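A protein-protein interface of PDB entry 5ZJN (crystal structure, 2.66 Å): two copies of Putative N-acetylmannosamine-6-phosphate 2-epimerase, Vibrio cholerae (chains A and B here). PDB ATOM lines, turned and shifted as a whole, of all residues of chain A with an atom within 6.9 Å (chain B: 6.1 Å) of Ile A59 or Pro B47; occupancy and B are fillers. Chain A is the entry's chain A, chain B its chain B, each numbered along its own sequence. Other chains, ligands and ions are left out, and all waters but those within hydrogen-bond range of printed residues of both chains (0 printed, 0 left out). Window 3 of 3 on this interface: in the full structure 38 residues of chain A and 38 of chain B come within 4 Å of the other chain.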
ATOM      1  N   ILE A  40     -20.430   4.013  17.385  1.00  0.00           N
ATOM      2  CA  ILE A  40     -19.793   5.311  17.185  1.00  0.00           C
ATOM      3  C   ILE A  40     -18.286   5.100  17.288  1.00  0.00           C
ATOM      4  O   ILE A  40     -17.675   5.262  18.345  1.00  0.00           O
ATOM      5  CB  ILE A  40     -20.311   6.340  18.184  1.00  0.00           C
ATOM      6  CG1 ILE A  40     -21.844   6.399  18.078  1.00  0.00           C
ATOM      7  CG2 ILE A  40     -19.674   7.716  17.914  1.00  0.00           C
ATOM      8  CD1 ILE A  40     -22.470   7.451  18.902  1.00  0.00           C
ATOM      9  N   ILE A  54     -17.433  12.549  19.057  1.00  0.00           N
ATOM     10  CA  ILE A  54     -18.050  11.277  19.407  1.00  0.00           C
ATOM     11  C   ILE A  54     -19.227  11.489  20.362  1.00  0.00           C
ATOM     12  O   ILE A  54     -20.312  10.921  20.176  1.00  0.00           O
ATOM     13  CB  ILE A  54     -16.984  10.323  19.973  1.00  0.00           C
ATOM     14  CG1 ILE A  54     -16.012   9.921  18.851  1.00  0.00           C
ATOM     15  CG2 ILE A  54     -17.627   9.092  20.634  1.00  0.00           C
ATOM     16  CD1 ILE A  54     -14.799   9.105  19.295  1.00  0.00           C
ATOM     17  N   VAL A  55     -19.039  12.316  21.389  1.00  0.00           N
ATOM     18  CA  VAL A  55     -20.130  12.595  22.323  1.00  0.00           C
ATOM     19  C   VAL A  55     -21.314  13.244  21.607  1.00  0.00           C
ATOM     20  O   VAL A  55     -22.469  12.837  21.783  1.00  0.00           O
ATOM     21  CB  VAL A  55     -19.626  13.503  23.454  1.00  0.00           C
ATOM     22  CG1 VAL A  55     -20.795  13.975  24.320  1.00  0.00           C
ATOM     23  CG2 VAL A  55     -18.512  12.835  24.259  1.00  0.00           C
ATOM     24  N   ALA A  56     -21.036  14.261  20.775  1.00  0.00           N
ATOM     25  CA  ALA A  56     -22.072  14.960  20.010  1.00  0.00           C
ATOM     26  C   ALA A  56     -22.863  14.008  19.123  1.00  0.00           C
ATOM     27  O   ALA A  56     -24.079  14.153  18.975  1.00  0.00           O
ATOM     28  CB  ALA A  56     -21.435  16.065  19.164  1.00  0.00           C
ATOM     29  N   MET A  57     -22.167  13.097  18.438  1.00  0.00           N
ATOM     30  CA  MET A  57     -22.851  12.046  17.692  1.00  0.00           C
ATOM     31  C   MET A  57     -23.674  11.159  18.624  1.00  0.00           C
ATOM     32  O   MET A  57     -24.761  10.701  18.259  1.00  0.00           O
ATOM     33  CB  MET A  57     -21.843  11.199  16.912  1.00  0.00           C
ATOM     34  CG  MET A  57     -21.168  11.906  15.750  1.00  0.00           C
ATOM     35  SD  MET A  57     -20.180  10.778  14.723  1.00  0.00           S
ATOM     36  CE  MET A  57     -18.624  10.790  15.597  1.00  0.00           C
ATOM     37  N   ALA A  58     -23.159  10.897  19.828  1.00  0.00           N
ATOM     38  CA  ALA A  58     -23.905  10.097  20.790  1.00  0.00           C
ATOM     39  C   ALA A  58     -25.180  10.800  21.206  1.00  0.00           C
ATOM     40  O   ALA A  58     -26.268  10.213  21.173  1.00  0.00           O
ATOM     41  CB  ALA A  58     -23.044   9.798  22.013  1.00  0.00           C
ATOM     42  N   ILE A  59     -25.073  12.076  21.565  1.00  0.00           N
ATOM     43  CA  ILE A  59     -26.267  12.853  21.889  1.00  0.00           C
ATOM     44  C   ILE A  59     -27.221  12.864  20.699  1.00  0.00           C
ATOM     45  O   ILE A  59     -28.444  12.791  20.857  1.00  0.00           O
ATOM     46  CB  ILE A  59     -25.876  14.281  22.323  1.00  0.00           C
ATOM     47  CG1 ILE A  59     -24.993  14.243  23.569  1.00  0.00           C
ATOM     48  CG2 ILE A  59     -27.099  15.044  22.687  1.00  0.00           C
ATOM     49  CD1 ILE A  59     -24.371  15.574  23.928  1.00  0.00           C
ATOM     50  N   ALA A  60     -26.667  12.901  19.489  1.00  0.00           N
ATOM     51  CA  ALA A  60     -27.480  13.090  18.297  1.00  0.00           C
ATOM     52  C   ALA A  60     -28.338  11.867  17.986  1.00  0.00           C
ATOM     53  O   ALA A  60     -29.535  11.998  17.702  1.00  0.00           O
ATOM     54  CB  ALA A  60     -26.568  13.445  17.117  1.00  0.00           C
ATOM     55  N   VAL A  61     -27.754  10.666  18.045  1.00  0.00           N
ATOM     56  CA  VAL A  61     -28.532   9.464  17.744  1.00  0.00           C
ATOM     57  C   VAL A  61     -29.531   9.171  18.853  1.00  0.00           C
ATOM     58  O   VAL A  61     -30.608   8.615  18.600  1.00  0.00           O
ATOM     59  CB  VAL A  61     -27.601   8.261  17.496  1.00  0.00           C
ATOM     60  CG1 VAL A  61     -26.706   8.524  16.291  1.00  0.00           C
ATOM     61  CG2 VAL A  61     -26.751   7.963  18.718  1.00  0.00           C
ATOM     62  N   GLU A  62     -29.220   9.555  20.088  1.00  0.00           N
ATOM     63  CA  GLU A  62     -30.203   9.367  21.142  1.00  0.00           C
ATOM     64  C   GLU A  62     -31.391  10.303  20.958  1.00  0.00           C
ATOM     65  O   GLU A  62     -32.543   9.885  21.122  1.00  0.00           O
ATOM     66  CB  GLU A  62     -29.551   9.564  22.511  1.00  0.00           C
ATOM     67  CG  GLU A  62     -30.550   9.902  23.651  1.00  0.00           C
ATOM     68  CD  GLU A  62     -29.870  10.185  25.010  1.00  0.00           C
ATOM     69  OE1 GLU A  62     -29.494  11.354  25.285  1.00  0.00           O
ATOM     70  OE2 GLU A  62     -29.710   9.212  25.809  1.00  0.00           O
ATOM     71  N   GLN A  63     -31.130  11.555  20.550  1.00  0.00           N
ATOM     72  CA  GLN A  63     -32.197  12.485  20.197  1.00  0.00           C
ATOM     73  C   GLN A  63     -33.048  11.952  19.044  1.00  0.00           C
ATOM     74  O   GLN A  63     -34.268  12.148  19.018  1.00  0.00           O
ATOM     75  CB  GLN A  63     -31.577  13.835  19.846  1.00  0.00           C
ATOM     76  CG  GLN A  63     -30.986  14.613  21.035  1.00  0.00           C
ATOM     77  CD  GLN A  63     -30.212  15.869  20.620  1.00  0.00           C
ATOM     78  OE1 GLN A  63     -29.896  16.059  19.450  1.00  0.00           O
ATOM     79  NE2 GLN A  63     -29.969  16.757  21.582  1.00  0.00           N
ATOM     80  N   ALA A  64     -32.431  11.265  18.089  1.00  0.00           N
ATOM     81  CA  ALA A  64     -33.143  10.659  16.967  1.00  0.00           C
ATOM     82  C   ALA A  64     -33.814   9.304  17.279  1.00  0.00           C
ATOM     83  O   ALA A  64     -34.449   8.735  16.384  1.00  0.00           O
ATOM     84  CB  ALA A  64     -32.191  10.491  15.785  1.00  0.00           C
ATOM     85  N   LEU A  69     -25.822   2.051  22.213  1.00  0.00           N
ATOM     86  CA  LEU A  69     -24.599   2.406  21.509  1.00  0.00           C
ATOM     87  C   LEU A  69     -23.485   1.408  21.794  1.00  0.00           C
ATOM     88  O   LEU A  69     -23.459   0.740  22.832  1.00  0.00           O
ATOM     89  CB  LEU A  69     -24.117   3.808  21.907  1.00  0.00           C
ATOM     90  CG  LEU A  69     -25.089   4.945  21.642  1.00  0.00           C
ATOM     91  CD1 LEU A  69     -24.560   6.277  22.142  1.00  0.00           C
ATOM     92  CD2 LEU A  69     -25.309   4.984  20.147  1.00  0.00           C
ATOM     93  N   VAL A  80     -19.196   9.580  27.010  1.00  0.00           N
ATOM     94  CA  VAL A  80     -20.540   9.413  26.470  1.00  0.00           C
ATOM     95  C   VAL A  80     -21.530   9.044  27.578  1.00  0.00           C
ATOM     96  O   VAL A  80     -22.680   9.490  27.565  1.00  0.00           O
ATOM     97  CB  VAL A  80     -20.539   8.388  25.325  1.00  0.00           C
ATOM     98  CG1 VAL A  80     -21.961   8.067  24.907  1.00  0.00           C
ATOM     99  CG2 VAL A  80     -19.764   8.929  24.154  1.00  0.00           C
ATOM    100  N   ALA A  83     -23.111  11.988  29.179  1.00  0.00           N
ATOM    101  CA  ALA A  83     -23.864  12.865  28.295  1.00  0.00           C
ATOM    102  C   ALA A  83     -25.165  12.257  27.800  1.00  0.00           C
ATOM    103  O   ALA A  83     -26.112  12.991  27.520  1.00  0.00           O
ATOM    104  CB  ALA A  83     -23.008  13.221  27.074  1.00  0.00           C
ATOM    105  N   VAL A  84     -25.229  10.935  27.670  1.00  0.00           N
ATOM    106  CA  VAL A  84     -26.467  10.273  27.285  1.00  0.00           C
ATOM    107  C   VAL A  84     -26.941   9.390  28.437  1.00  0.00           C
ATOM    108  O   VAL A  84     -26.253   9.268  29.458  1.00  0.00           O
ATOM    109  CB  VAL A  84     -26.284   9.481  25.974  1.00  0.00           C
ATOM    110  CG1 VAL A  84     -25.794  10.420  24.865  1.00  0.00           C
ATOM    111  CG2 VAL A  84     -25.325   8.325  26.159  1.00  0.00           C
ATOM    112  N   GLY B  45     -30.345  22.593  14.514  1.00  0.00           N
ATOM    113  CA  GLY B  45     -30.549  22.354  15.932  1.00  0.00           C
ATOM    114  C   GLY B  45     -29.813  21.157  16.514  1.00  0.00           C
ATOM    115  O   GLY B  45     -29.884  20.930  17.733  1.00  0.00           O
ATOM    116  N   SER B  46     -29.114  20.389  15.690  1.00  0.00           N
ATOM    117  CA  SER B  46     -28.407  19.210  16.143  1.00  0.00           C
ATOM    118  C   SER B  46     -27.197  19.604  16.981  1.00  0.00           C
ATOM    119  O   SER B  46     -26.653  20.697  16.826  1.00  0.00           O
ATOM    120  CB  SER B  46     -27.962  18.405  14.928  1.00  0.00           C
ATOM    121  OG  SER B  46     -27.086  17.354  15.265  1.00  0.00           O
ATOM    122  N   PRO B  47     -26.731  18.720  17.866  1.00  0.00           N
ATOM    123  CA  PRO B  47     -25.389  18.925  18.436  1.00  0.00           C
ATOM    124  C   PRO B  47     -24.341  18.976  17.356  1.00  0.00           C
ATOM    125  O   PRO B  47     -23.242  19.489  17.592  1.00  0.00           O
ATOM    126  CB  PRO B  47     -25.186  17.702  19.343  1.00  0.00           C
ATOM    127  CG  PRO B  47     -26.544  17.185  19.602  1.00  0.00           C
ATOM    128  CD  PRO B  47     -27.361  17.491  18.385  1.00  0.00           C
ATOM    129  N   LEU B  48     -24.662  18.451  16.172  1.00  0.00           N
ATOM    130  CA  LEU B  48     -23.755  18.367  15.042  1.00  0.00           C
ATOM    131  C   LEU B  48     -23.808  19.587  14.133  1.00  0.00           C
ATOM    132  O   LEU B  48     -22.969  19.707  13.235  1.00  0.00           O
ATOM    133  CB  LEU B  48     -24.054  17.102  14.224  1.00  0.00           C
ATOM    134  CG  LEU B  48     -23.972  15.780  14.992  1.00  0.00           C
ATOM    135  CD1 LEU B  48     -24.466  14.617  14.144  1.00  0.00           C
ATOM    136  CD2 LEU B  48     -22.558  15.548  15.507  1.00  0.00           C
ATOM    137  N   ASP B  49     -24.767  20.491  14.337  1.00  0.00           N
ATOM    138  CA  ASP B  49     -24.867  21.693  13.517  1.00  0.00           C
ATOM    139  C   ASP B  49     -23.901  22.769  14.033  1.00  0.00           C
ATOM    140  O   ASP B  49     -24.294  23.856  14.451  1.00  0.00           O
ATOM    141  CB  ASP B  49     -26.308  22.191  13.486  1.00  0.00           C
ATOM    142  CG  ASP B  49     -26.537  23.257  12.413  1.00  0.00           C
ATOM    143  OD1 ASP B  49     -25.664  23.392  11.536  1.00  0.00           O
ATOM    144  OD2 ASP B  49     -27.582  23.942  12.450  1.00  0.00           O
ATOM    145  N   LYS B  50     -22.603  22.445  13.988  1.00  0.00           N
ATOM    146  CA  LYS B  50     -21.563  23.363  14.431  1.00  0.00           C
ATOM    147  C   LYS B  50     -20.476  23.492  13.371  1.00  0.00           C
ATOM    148  O   LYS B  50     -20.105  22.507  12.724  1.00  0.00           O
ATOM    149  CB  LYS B  50     -20.961  22.942  15.771  1.00  0.00           C
ATOM    150  CG  LYS B  50     -21.492  23.791  16.943  1.00  0.00           C
ATOM    151  CD  LYS B  50     -21.040  23.280  18.325  1.00  0.00           C
ATOM    152  CE  LYS B  50     -19.526  23.360  18.538  1.00  0.00           C
ATOM    153  NZ  LYS B  50     -19.135  22.845  19.885  1.00  0.00           N
ATOM    154  N   PHE B  53     -17.517  21.124  13.489  1.00  0.00           N
ATOM    155  CA  PHE B  53     -17.757  19.754  13.057  1.00  0.00           C
ATOM    156  C   PHE B  53     -17.941  19.700  11.553  1.00  0.00           C
ATOM    157  O   PHE B  53     -17.596  18.693  10.918  1.00  0.00           O
ATOM    158  CB  PHE B  53     -18.991  19.164  13.760  1.00  0.00           C
ATOM    159  CG  PHE B  53     -18.970  19.279  15.285  1.00  0.00           C
ATOM    160  CD1 PHE B  53     -17.848  19.723  15.974  1.00  0.00           C
ATOM    161  CD2 PHE B  53     -20.091  18.959  16.025  1.00  0.00           C
ATOM    162  CE1 PHE B  53     -17.846  19.840  17.371  1.00  0.00           C
ATOM    163  CE2 PHE B  53     -20.082  19.069  17.419  1.00  0.00           C
ATOM    164  CZ  PHE B  53     -18.949  19.514  18.085  1.00  0.00           C
ATOM    165  N   GLU B 233     -28.877  11.860  12.192  1.00  0.00           N
ATOM    166  CA  GLU B 233     -30.227  11.600  12.713  1.00  0.00           C
ATOM    167  C   GLU B 233     -31.138  10.990  11.652  1.00  0.00           C
ATOM    168  O   GLU B 233     -31.904  10.065  11.941  1.00  0.00           O
ATOM    169  CB  GLU B 233     -30.859  12.884  13.261  1.00  0.00           C
ATOM    170  CG  GLU B 233     -30.271  13.425  14.572  1.00  0.00           C
ATOM    171  CD  GLU B 233     -29.159  14.434  14.363  1.00  0.00           C
ATOM    172  OE1 GLU B 233     -28.495  14.365  13.311  1.00  0.00           O
ATOM    173  OE2 GLU B 233     -28.951  15.284  15.255  1.00  0.00           O
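OG of Ser B46 lies within hydrogen-bond range of N of Leu B48, at 2.8 Å.
The side-chain carboxylate (OE2) of Glu B233 is in hydrogen-bond range of the side-chain hydroxyl (OG) of Ser B46, at 2.8 Å.
Among the printed residues, pairs that only touch across the chains: Gln A63 with Pro B47 (3.1 Å), Ala A60 with Glu B233 (3.5 Å), Ala A64 with Glu B233 (3.7 Å), Ala A56 with Phe B53 (3.7 Å), Ala A56 with Pro B47 (3.7 Å), Ile A59 with Pro B47 (3.8 Å), Ala A60 with Leu B48 (3.8 Å), Met A57 with Leu B48 (3.8 Å) and Ala A56 with Leu B48 (3.9 Å).
Of the printed residues of chain B, Met A57 touches Leu B48.
Ile A59 touches just one residue of chain B: Pro B47 (3.8 Å).
Of the printed residues of chain B, Ala A60 touches Leu B48 (3.8 Å) and Glu B233 (3.5 Å).
Of the printed residues of chain B, Gln A63 touches Pro B47 (3.1 Å).
Pro B47 touches just these residues of chain A: Ala A56, Ile A59 and Gln A63.
Of the printed residues of chain A, Leu B48 touches Ala A56 (3.9 Å), Met A57 (3.8 Å) and Ala A60 (3.8 Å).
Of the printed residues of chain A, Phe B53 touches Ala A56 (3.7 Å).
The nearest printed residue of chain B that does not touch Ala A64 is Pro B47 (8.0 Å).
Of the 8 printed residues of chain B, 4 touch a printed residue of chain A.
Hydrophobic or aromatic side chains of chain B within 4 Å of the printed part of chain A: Pro B47, Leu B48 and Phe B53.
Of the 16 printed residues of chain A, 6 touch a printed residue of chain B.
Printed residues of chain A that touch a printed residue of chain B: Ala A56, Met A57, Ile A59, Ala A60, Gln A63 and Ala A64.
Among the printed residues, no Asp or Glu carboxylate lies within 4 Å of a Lys or Arg side-chain nitrogen of the other chain.
No position is printed for both chains.
Of the 9 pairs that touch across the chains among the printed residues, none has its exchanged pair printed and touching as well.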
